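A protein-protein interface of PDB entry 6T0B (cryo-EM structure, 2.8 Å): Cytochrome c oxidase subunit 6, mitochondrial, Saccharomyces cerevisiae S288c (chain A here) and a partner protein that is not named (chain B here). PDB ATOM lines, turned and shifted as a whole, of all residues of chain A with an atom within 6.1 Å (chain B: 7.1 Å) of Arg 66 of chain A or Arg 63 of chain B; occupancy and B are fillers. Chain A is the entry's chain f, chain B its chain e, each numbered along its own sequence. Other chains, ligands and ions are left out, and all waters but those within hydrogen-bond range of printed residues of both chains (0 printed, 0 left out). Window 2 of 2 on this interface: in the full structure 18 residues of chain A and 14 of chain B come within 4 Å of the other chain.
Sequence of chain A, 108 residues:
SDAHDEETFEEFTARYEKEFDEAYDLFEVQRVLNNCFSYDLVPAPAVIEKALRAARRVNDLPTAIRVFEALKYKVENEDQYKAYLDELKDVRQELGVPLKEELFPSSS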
ATOM      1  N   LEU A  33      -0.560  26.268 -31.727  1.00  0.00           N
ATOM      2  CA  LEU A  33      -0.296  24.919 -31.243  1.00  0.00           C
ATOM      3  C   LEU A  33      -1.493  24.010 -31.456  1.00  0.00           C
ATOM      4  O   LEU A  33      -1.333  22.839 -31.824  1.00  0.00           O
ATOM      5  CB  LEU A  33       0.075  24.988 -29.771  1.00  0.00           C
ATOM      6  CG  LEU A  33       0.347  23.702 -29.026  1.00  0.00           C
ATOM      7  CD1 LEU A  33       1.606  23.073 -29.544  1.00  0.00           C
ATOM      8  CD2 LEU A  33       0.491  24.064 -27.589  1.00  0.00           C
ATOM      9  N   LEU A  61       3.751  28.598 -18.485  1.00  0.00           N
ATOM     10  CA  LEU A  61       4.316  27.292 -18.177  1.00  0.00           C
ATOM     11  C   LEU A  61       3.392  26.102 -18.454  1.00  0.00           C
ATOM     12  O   LEU A  61       3.892  25.095 -18.966  1.00  0.00           O
ATOM     13  CB  LEU A  61       4.802  27.289 -16.723  1.00  0.00           C
ATOM     14  CG  LEU A  61       5.349  26.019 -16.082  1.00  0.00           C
ATOM     15  CD1 LEU A  61       6.486  25.452 -16.870  1.00  0.00           C
ATOM     16  CD2 LEU A  61       5.798  26.336 -14.685  1.00  0.00           C
ATOM     17  N   PRO A  62       2.082  26.123 -18.142  1.00  0.00           N
ATOM     18  CA  PRO A  62       1.275  24.937 -18.446  1.00  0.00           C
ATOM     19  C   PRO A  62       1.072  24.653 -19.920  1.00  0.00           C
ATOM     20  O   PRO A  62       0.735  23.513 -20.252  1.00  0.00           O
ATOM     21  CB  PRO A  62      -0.056  25.240 -17.760  1.00  0.00           C
ATOM     22  CG  PRO A  62      -0.066  26.654 -17.579  1.00  0.00           C
ATOM     23  CD  PRO A  62       1.299  26.997 -17.250  1.00  0.00           C
ATOM     24  N   THR A  63       1.273  25.617 -20.816  1.00  0.00           N
ATOM     25  CA  THR A  63       1.230  25.285 -22.235  1.00  0.00           C
ATOM     26  C   THR A  63       2.436  24.453 -22.648  1.00  0.00           C
ATOM     27  O   THR A  63       2.311  23.556 -23.485  1.00  0.00           O
ATOM     28  CB  THR A  63       1.138  26.551 -23.069  1.00  0.00           C
ATOM     29  OG1 THR A  63       0.198  27.436 -22.462  1.00  0.00           O
ATOM     30  CG2 THR A  63       0.665  26.236 -24.464  1.00  0.00           C
ATOM     31  N   ALA A  64       3.593  24.685 -22.034  1.00  0.00           N
ATOM     32  CA  ALA A  64       4.749  23.861 -22.343  1.00  0.00           C
ATOM     33  C   ALA A  64       4.671  22.483 -21.702  1.00  0.00           C
ATOM     34  O   ALA A  64       5.486  21.618 -22.026  1.00  0.00           O
ATOM     35  CB  ALA A  64       6.027  24.569 -21.917  1.00  0.00           C
ATOM     36  N   ILE A  65       3.733  22.261 -20.788  1.00  0.00           N
ATOM     37  CA  ILE A  65       3.438  20.919 -20.302  1.00  0.00           C
ATOM     38  C   ILE A  65       2.395  20.248 -21.175  1.00  0.00           C
ATOM     39  O   ILE A  65       2.470  19.047 -21.464  1.00  0.00           O
ATOM     40  CB  ILE A  65       2.968  21.002 -18.844  1.00  0.00           C
ATOM     41  CG1 ILE A  65       3.920  21.862 -18.035  1.00  0.00           C
ATOM     42  CG2 ILE A  65       2.874  19.633 -18.239  1.00  0.00           C
ATOM     43  CD1 ILE A  65       3.393  22.209 -16.689  1.00  0.00           C
ATOM     44  N   ARG A  66       1.420  21.034 -21.612  1.00  0.00           N
ATOM     45  CA  ARG A  66       0.374  20.525 -22.473  1.00  0.00           C
ATOM     46  C   ARG A  66       0.895  20.178 -23.854  1.00  0.00           C
ATOM     47  O   ARG A  66       0.260  19.383 -24.546  1.00  0.00           O
ATOM     48  CB  ARG A  66      -0.746  21.547 -22.561  1.00  0.00           C
ATOM     49  CG  ARG A  66      -2.078  20.987 -22.972  1.00  0.00           C
ATOM     50  CD  ARG A  66      -2.677  20.118 -21.907  1.00  0.00           C
ATOM     51  NE  ARG A  66      -4.105  19.964 -22.124  1.00  0.00           N
ATOM     52  CZ  ARG A  66      -4.938  19.414 -21.256  1.00  0.00           C
ATOM     53  NH1 ARG A  66      -4.483  18.954 -20.104  1.00  0.00           N
ATOM     54  NH2 ARG A  66      -6.223  19.324 -21.541  1.00  0.00           N
ATOM     55  N   VAL A  67       2.039  20.737 -24.256  1.00  0.00           N
ATOM     56  CA  VAL A  67       2.717  20.300 -25.476  1.00  0.00           C
ATOM     57  C   VAL A  67       3.077  18.822 -25.386  1.00  0.00           C
ATOM     58  O   VAL A  67       2.800  18.034 -26.302  1.00  0.00           O
ATOM     59  CB  VAL A  67       3.960  21.169 -25.727  1.00  0.00           C
ATOM     60  CG1 VAL A  67       4.940  20.478 -26.612  1.00  0.00           C
ATOM     61  CG2 VAL A  67       3.574  22.471 -26.344  1.00  0.00           C
ATOM     62  N   PHE A  68       3.654  18.411 -24.260  1.00  0.00           N
ATOM     63  CA  PHE A  68       4.045  17.018 -24.122  1.00  0.00           C
ATOM     64  C   PHE A  68       2.847  16.119 -23.881  1.00  0.00           C
ATOM     65  O   PHE A  68       2.841  14.977 -24.345  1.00  0.00           O
ATOM     66  CB  PHE A  68       5.068  16.873 -23.011  1.00  0.00           C
ATOM     67  CG  PHE A  68       6.422  17.367 -23.387  1.00  0.00           C
ATOM     68  CD1 PHE A  68       7.185  16.685 -24.303  1.00  0.00           C
ATOM     69  CD2 PHE A  68       6.929  18.519 -22.834  1.00  0.00           C
ATOM     70  CE1 PHE A  68       8.429  17.130 -24.644  1.00  0.00           C
ATOM     71  CE2 PHE A  68       8.173  18.972 -23.189  1.00  0.00           C
ATOM     72  CZ  PHE A  68       8.921  18.271 -24.089  1.00  0.00           C
ATOM     73  N   GLU A  69       1.819  16.615 -23.188  1.00  0.00           N
ATOM     74  CA  GLU A  69       0.576  15.849 -23.081  1.00  0.00           C
ATOM     75  C   GLU A  69      -0.068  15.643 -24.446  1.00  0.00           C
ATOM     76  O   GLU A  69      -0.595  14.561 -24.744  1.00  0.00           O
ATOM     77  CB  GLU A  69      -0.407  16.548 -22.154  1.00  0.00           C
ATOM     78  CG  GLU A  69       0.099  16.784 -20.767  1.00  0.00           C
ATOM     79  CD  GLU A  69      -0.840  17.644 -19.963  1.00  0.00           C
ATOM     80  OE1 GLU A  69      -2.065  17.414 -20.026  1.00  0.00           O
ATOM     81  OE2 GLU A  69      -0.359  18.561 -19.268  1.00  0.00           O
ATOM     82  N   ALA A  70       0.003  16.660 -25.298  1.00  0.00           N
ATOM     83  CA  ALA A  70      -0.556  16.572 -26.632  1.00  0.00           C
ATOM     84  C   ALA A  70       0.210  15.585 -27.492  1.00  0.00           C
ATOM     85  O   ALA A  70      -0.399  14.805 -28.227  1.00  0.00           O
ATOM     86  CB  ALA A  70      -0.562  17.949 -27.281  1.00  0.00           C
ATOM     87  N   LEU A  71       1.538  15.580 -27.415  1.00  0.00           N
ATOM     88  CA  LEU A  71       2.231  14.610 -28.252  1.00  0.00           C
ATOM     89  C   LEU A  71       2.189  13.214 -27.667  1.00  0.00           C
ATOM     90  O   LEU A  71       2.362  12.249 -28.413  1.00  0.00           O
ATOM     91  CB  LEU A  71       3.669  15.029 -28.551  1.00  0.00           C
ATOM     92  CG  LEU A  71       4.769  15.236 -27.533  1.00  0.00           C
ATOM     93  CD1 LEU A  71       5.565  13.982 -27.315  1.00  0.00           C
ATOM     94  CD2 LEU A  71       5.672  16.313 -28.056  1.00  0.00           C
ATOM     95  N   LYS A 100       3.841  15.984 -17.310  1.00  0.00           N
ATOM     96  CA  LYS A 100       2.658  15.942 -16.462  1.00  0.00           C
ATOM     97  C   LYS A 100       2.627  14.697 -15.597  1.00  0.00           C
ATOM     98  O   LYS A 100       2.109  14.737 -14.477  1.00  0.00           O
ATOM     99  CB  LYS A 100       1.401  16.019 -17.318  1.00  0.00           C
ATOM    100  CG  LYS A 100       0.121  16.191 -16.543  1.00  0.00           C
ATOM    101  CD  LYS A 100      -0.956  15.340 -17.143  1.00  0.00           C
ATOM    102  CE  LYS A 100      -2.219  15.421 -16.349  1.00  0.00           C
ATOM    103  NZ  LYS A 100      -2.009  14.915 -14.978  1.00  0.00           N
ATOM    104  N   TRP B  53      -1.189  24.744 -13.393  1.00  0.00           N
ATOM    105  CA  TRP B  53      -1.749  23.788 -14.334  1.00  0.00           C
ATOM    106  C   TRP B  53      -3.218  23.547 -14.057  1.00  0.00           C
ATOM    107  O   TRP B  53      -3.994  23.327 -14.990  1.00  0.00           O
ATOM    108  CB  TRP B  53      -0.990  22.468 -14.286  1.00  0.00           C
ATOM    109  CG  TRP B  53      -1.406  21.541 -15.373  1.00  0.00           C
ATOM    110  CD1 TRP B  53      -0.860  21.444 -16.609  1.00  0.00           C
ATOM    111  CD2 TRP B  53      -2.472  20.589 -15.334  1.00  0.00           C
ATOM    112  NE1 TRP B  53      -1.509  20.492 -17.344  1.00  0.00           N
ATOM    113  CE2 TRP B  53      -2.509  19.958 -16.581  1.00  0.00           C
ATOM    114  CE3 TRP B  53      -3.400  20.213 -14.364  1.00  0.00           C
ATOM    115  CZ2 TRP B  53      -3.427  18.973 -16.881  1.00  0.00           C
ATOM    116  CZ3 TRP B  53      -4.309  19.245 -14.666  1.00  0.00           C
ATOM    117  CH2 TRP B  53      -4.320  18.634 -15.910  1.00  0.00           C
ATOM    118  N   SER B  56      -5.182  26.590 -15.294  1.00  0.00           N
ATOM    119  CA  SER B  56      -5.215  26.684 -16.741  1.00  0.00           C
ATOM    120  C   SER B  56      -5.875  25.491 -17.412  1.00  0.00           C
ATOM    121  O   SER B  56      -6.423  25.642 -18.501  1.00  0.00           O
ATOM    122  CB  SER B  56      -3.803  26.848 -17.287  1.00  0.00           C
ATOM    123  OG  SER B  56      -3.775  26.511 -18.652  1.00  0.00           O
ATOM    124  N   TYR B  57      -5.839  24.307 -16.811  1.00  0.00           N
ATOM    125  CA  TYR B  57      -6.259  23.122 -17.548  1.00  0.00           C
ATOM    126  C   TYR B  57      -7.071  22.131 -16.729  1.00  0.00           C
ATOM    127  O   TYR B  57      -7.250  20.997 -17.170  1.00  0.00           O
ATOM    128  CB  TYR B  57      -5.064  22.368 -18.097  1.00  0.00           C
ATOM    129  CG  TYR B  57      -4.404  23.016 -19.267  1.00  0.00           C
ATOM    130  CD1 TYR B  57      -5.091  23.224 -20.438  1.00  0.00           C
ATOM    131  CD2 TYR B  57      -3.085  23.404 -19.204  1.00  0.00           C
ATOM    132  CE1 TYR B  57      -4.492  23.817 -21.506  1.00  0.00           C
ATOM    133  CE2 TYR B  57      -2.475  23.993 -20.270  1.00  0.00           C
ATOM    134  CZ  TYR B  57      -3.181  24.195 -21.415  1.00  0.00           C
ATOM    135  OH  TYR B  57      -2.569  24.787 -22.483  1.00  0.00           O
ATOM    136  N   GLY B  58      -7.557  22.500 -15.556  1.00  0.00           N
ATOM    137  CA  GLY B  58      -8.250  21.551 -14.720  1.00  0.00           C
ATOM    138  C   GLY B  58      -9.658  21.301 -15.189  1.00  0.00           C
ATOM    139  O   GLY B  58     -10.160  21.920 -16.121  1.00  0.00           O
ATOM    140  N   GLU B  59     -10.330  20.400 -14.483  1.00  0.00           N
ATOM    141  CA  GLU B  59     -11.677  19.948 -14.824  1.00  0.00           C
ATOM    142  C   GLU B  59     -12.716  20.722 -14.021  1.00  0.00           C
ATOM    143  O   GLU B  59     -13.695  20.203 -13.492  1.00  0.00           O
ATOM    144  CB  GLU B  59     -11.761  18.435 -14.627  1.00  0.00           C
ATOM    145  CG  GLU B  59     -12.995  17.637 -15.139  1.00  0.00           C
ATOM    146  CD  GLU B  59     -13.230  17.704 -16.644  1.00  0.00           C
ATOM    147  OE1 GLU B  59     -12.308  18.085 -17.403  1.00  0.00           O
ATOM    148  OE2 GLU B  59     -14.338  17.310 -17.072  1.00  0.00           O
ATOM    149  N   TRP B  60     -12.463  22.010 -13.882  1.00  0.00           N
ATOM    150  CA  TRP B  60     -13.401  22.981 -13.358  1.00  0.00           C
ATOM    151  C   TRP B  60     -13.882  23.874 -14.487  1.00  0.00           C
ATOM    152  O   TRP B  60     -13.373  23.815 -15.603  1.00  0.00           O
ATOM    153  CB  TRP B  60     -12.746  23.831 -12.273  1.00  0.00           C
ATOM    154  CG  TRP B  60     -11.663  24.694 -12.800  1.00  0.00           C
ATOM    155  CD1 TRP B  60     -10.417  24.305 -13.147  1.00  0.00           C
ATOM    156  CD2 TRP B  60     -11.727  26.095 -13.048  1.00  0.00           C
ATOM    157  NE1 TRP B  60      -9.699  25.368 -13.601  1.00  0.00           N
ATOM    158  CE2 TRP B  60     -10.485  26.483 -13.550  1.00  0.00           C
ATOM    159  CE3 TRP B  60     -12.721  27.060 -12.899  1.00  0.00           C
ATOM    160  CZ2 TRP B  60     -10.204  27.786 -13.900  1.00  0.00           C
ATOM    161  CZ3 TRP B  60     -12.442  28.346 -13.247  1.00  0.00           C
ATOM    162  CH2 TRP B  60     -11.197  28.702 -13.743  1.00  0.00           C
ATOM    163  N   GLY B  61     -14.880  24.693 -14.179  1.00  0.00           N
ATOM    164  CA  GLY B  61     -15.306  25.769 -15.039  1.00  0.00           C
ATOM    165  C   GLY B  61     -15.863  25.323 -16.366  1.00  0.00           C
ATOM    166  O   GLY B  61     -16.837  24.580 -16.437  1.00  0.00           O
ATOM    167  N   PRO B  62     -15.257  25.793 -17.452  1.00  0.00           N
ATOM    168  CA  PRO B  62     -15.684  25.342 -18.774  1.00  0.00           C
ATOM    169  C   PRO B  62     -15.396  23.887 -19.051  1.00  0.00           C
ATOM    170  O   PRO B  62     -16.099  23.286 -19.866  1.00  0.00           O
ATOM    171  CB  PRO B  62     -14.895  26.245 -19.716  1.00  0.00           C
ATOM    172  CG  PRO B  62     -14.538  27.407 -18.921  1.00  0.00           C
ATOM    173  CD  PRO B  62     -14.327  26.923 -17.540  1.00  0.00           C
ATOM    174  N   ARG B  63     -14.393  23.295 -18.416  1.00  0.00           N
ATOM    175  CA  ARG B  63     -14.047  21.924 -18.737  1.00  0.00           C
ATOM    176  C   ARG B  63     -14.893  20.916 -18.003  1.00  0.00           C
ATOM    177  O   ARG B  63     -14.765  19.739 -18.319  1.00  0.00           O
ATOM    178  CB  ARG B  63     -12.582  21.664 -18.434  1.00  0.00           C
ATOM    179  CG  ARG B  63     -11.678  22.184 -19.512  1.00  0.00           C
ATOM    180  CD  ARG B  63     -10.271  21.697 -19.399  1.00  0.00           C
ATOM    181  NE  ARG B  63      -9.392  22.648 -20.051  1.00  0.00           N
ATOM    182  CZ  ARG B  63      -8.872  22.465 -21.246  1.00  0.00           C
ATOM    183  NH1 ARG B  63      -8.093  23.379 -21.769  1.00  0.00           N
ATOM    184  NH2 ARG B  63      -9.120  21.351 -21.902  1.00  0.00           N
ATOM    185  N   ARG B  64     -15.731  21.373 -17.072  1.00  0.00           N
ATOM    186  CA  ARG B  64     -16.621  20.558 -16.258  1.00  0.00           C
ATOM    187  C   ARG B  64     -17.435  19.601 -17.121  1.00  0.00           C
ATOM    188  O   ARG B  64     -18.028  20.030 -18.116  1.00  0.00           O
ATOM    189  CB  ARG B  64     -17.542  21.502 -15.498  1.00  0.00           C
ATOM    190  CG  ARG B  64     -18.502  20.880 -14.542  1.00  0.00           C
ATOM    191  CD  ARG B  64     -19.462  21.917 -14.077  1.00  0.00           C
ATOM    192  NE  ARG B  64     -18.788  23.163 -13.722  1.00  0.00           N
ATOM    193  CZ  ARG B  64     -18.244  23.407 -12.531  1.00  0.00           C
ATOM    194  NH1 ARG B  64     -18.283  22.483 -11.582  1.00  0.00           N
ATOM    195  NH2 ARG B  64     -17.658  24.572 -12.284  1.00  0.00           N
ATOM    196  N   PRO B  65     -17.446  18.310 -16.810  1.00  0.00           N
ATOM    197  CA  PRO B  65     -17.887  17.314 -17.783  1.00  0.00           C
ATOM    198  C   PRO B  65     -19.394  17.263 -17.925  1.00  0.00           C
ATOM    199  O   PRO B  65     -20.151  17.781 -17.107  1.00  0.00           O
ATOM    200  CB  PRO B  65     -17.368  16.013 -17.183  1.00  0.00           C
ATOM    201  CG  PRO B  65     -17.515  16.242 -15.753  1.00  0.00           C
ATOM    202  CD  PRO B  65     -17.140  17.675 -15.520  1.00  0.00           C
ATOM    203  N   VAL B  66     -19.825  16.607 -18.996  1.00  0.00           N
ATOM    204  CA  VAL B  66     -21.253  16.444 -19.201  1.00  0.00           C
ATOM    205  C   VAL B  66     -21.792  15.335 -18.303  1.00  0.00           C
ATOM    206  O   VAL B  66     -22.947  15.383 -17.867  1.00  0.00           O
ATOM    207  CB  VAL B  66     -21.526  16.232 -20.705  1.00  0.00           C
ATOM    208  CG1 VAL B  66     -20.807  15.017 -21.222  1.00  0.00           C
ATOM    209  CG2 VAL B  66     -23.005  16.153 -21.001  1.00  0.00           C
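OE1 of Glu 69 of chain A is in salt-bridge range of NH1 of Arg 66 of chain A, 2.9 Å away.
Ser 56 of chain B touches Pro 62 of chain A (CB to CG, 3.8 Å). Pro 62 of chain A touches Tyr 57 of chain B (O to CE2, 3.2 Å). Tyr 57 of chain B touches Thr 63 of chain A. Arg 66 of chain A touches Trp 53 of chain B. Arg 66 of chain A touches Tyr 57 of chain B. Arg 63 of chain B touches Arg 66 of chain A. Lys 100 of chain A touches Trp 53 of chain B.
Arg 66 of chain A touches just these residues of chain B: Trp 53 (3.4 Å), Tyr 57 (3.7 Å) and Arg 63 (3.6 Å). Arg 63 of chain B touches one residue of chain A. Of the printed residues of chain B, Thr 63 of chain A touches Tyr 57 (3.8 Å). Of the printed residues of chain A, Trp 53 of chain B touches Arg 66, Glu 69 and Lys 100. Printed residues of chain B within 4 Å of Pro 62 of chain A: Ser 56 (3.8 Å) and Tyr 57 (3.2 Å). Of the printed residues of chain B, Lys 100 of chain A touches Trp 53. Leu 71 of chain A touches none of the printed residues of chain B. Pro 65 of chain B touches none of the printed residues of chain A. The nearest printed residue of chain A that does not touch Arg 63 of chain B is Glu 69 of chain A (8.3 Å).
The indole nitrogen of Trp 53 of chain B sits at hydrogen-bond distance from the side-chain carboxylate of Glu 69 of chain A.
Of the 13 printed residues of chain A, 5 touch a printed residue of chain B. Hydrophobic or aromatic side chains of chain B that line the printed part of chain A: Trp 53 and Tyr 57.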
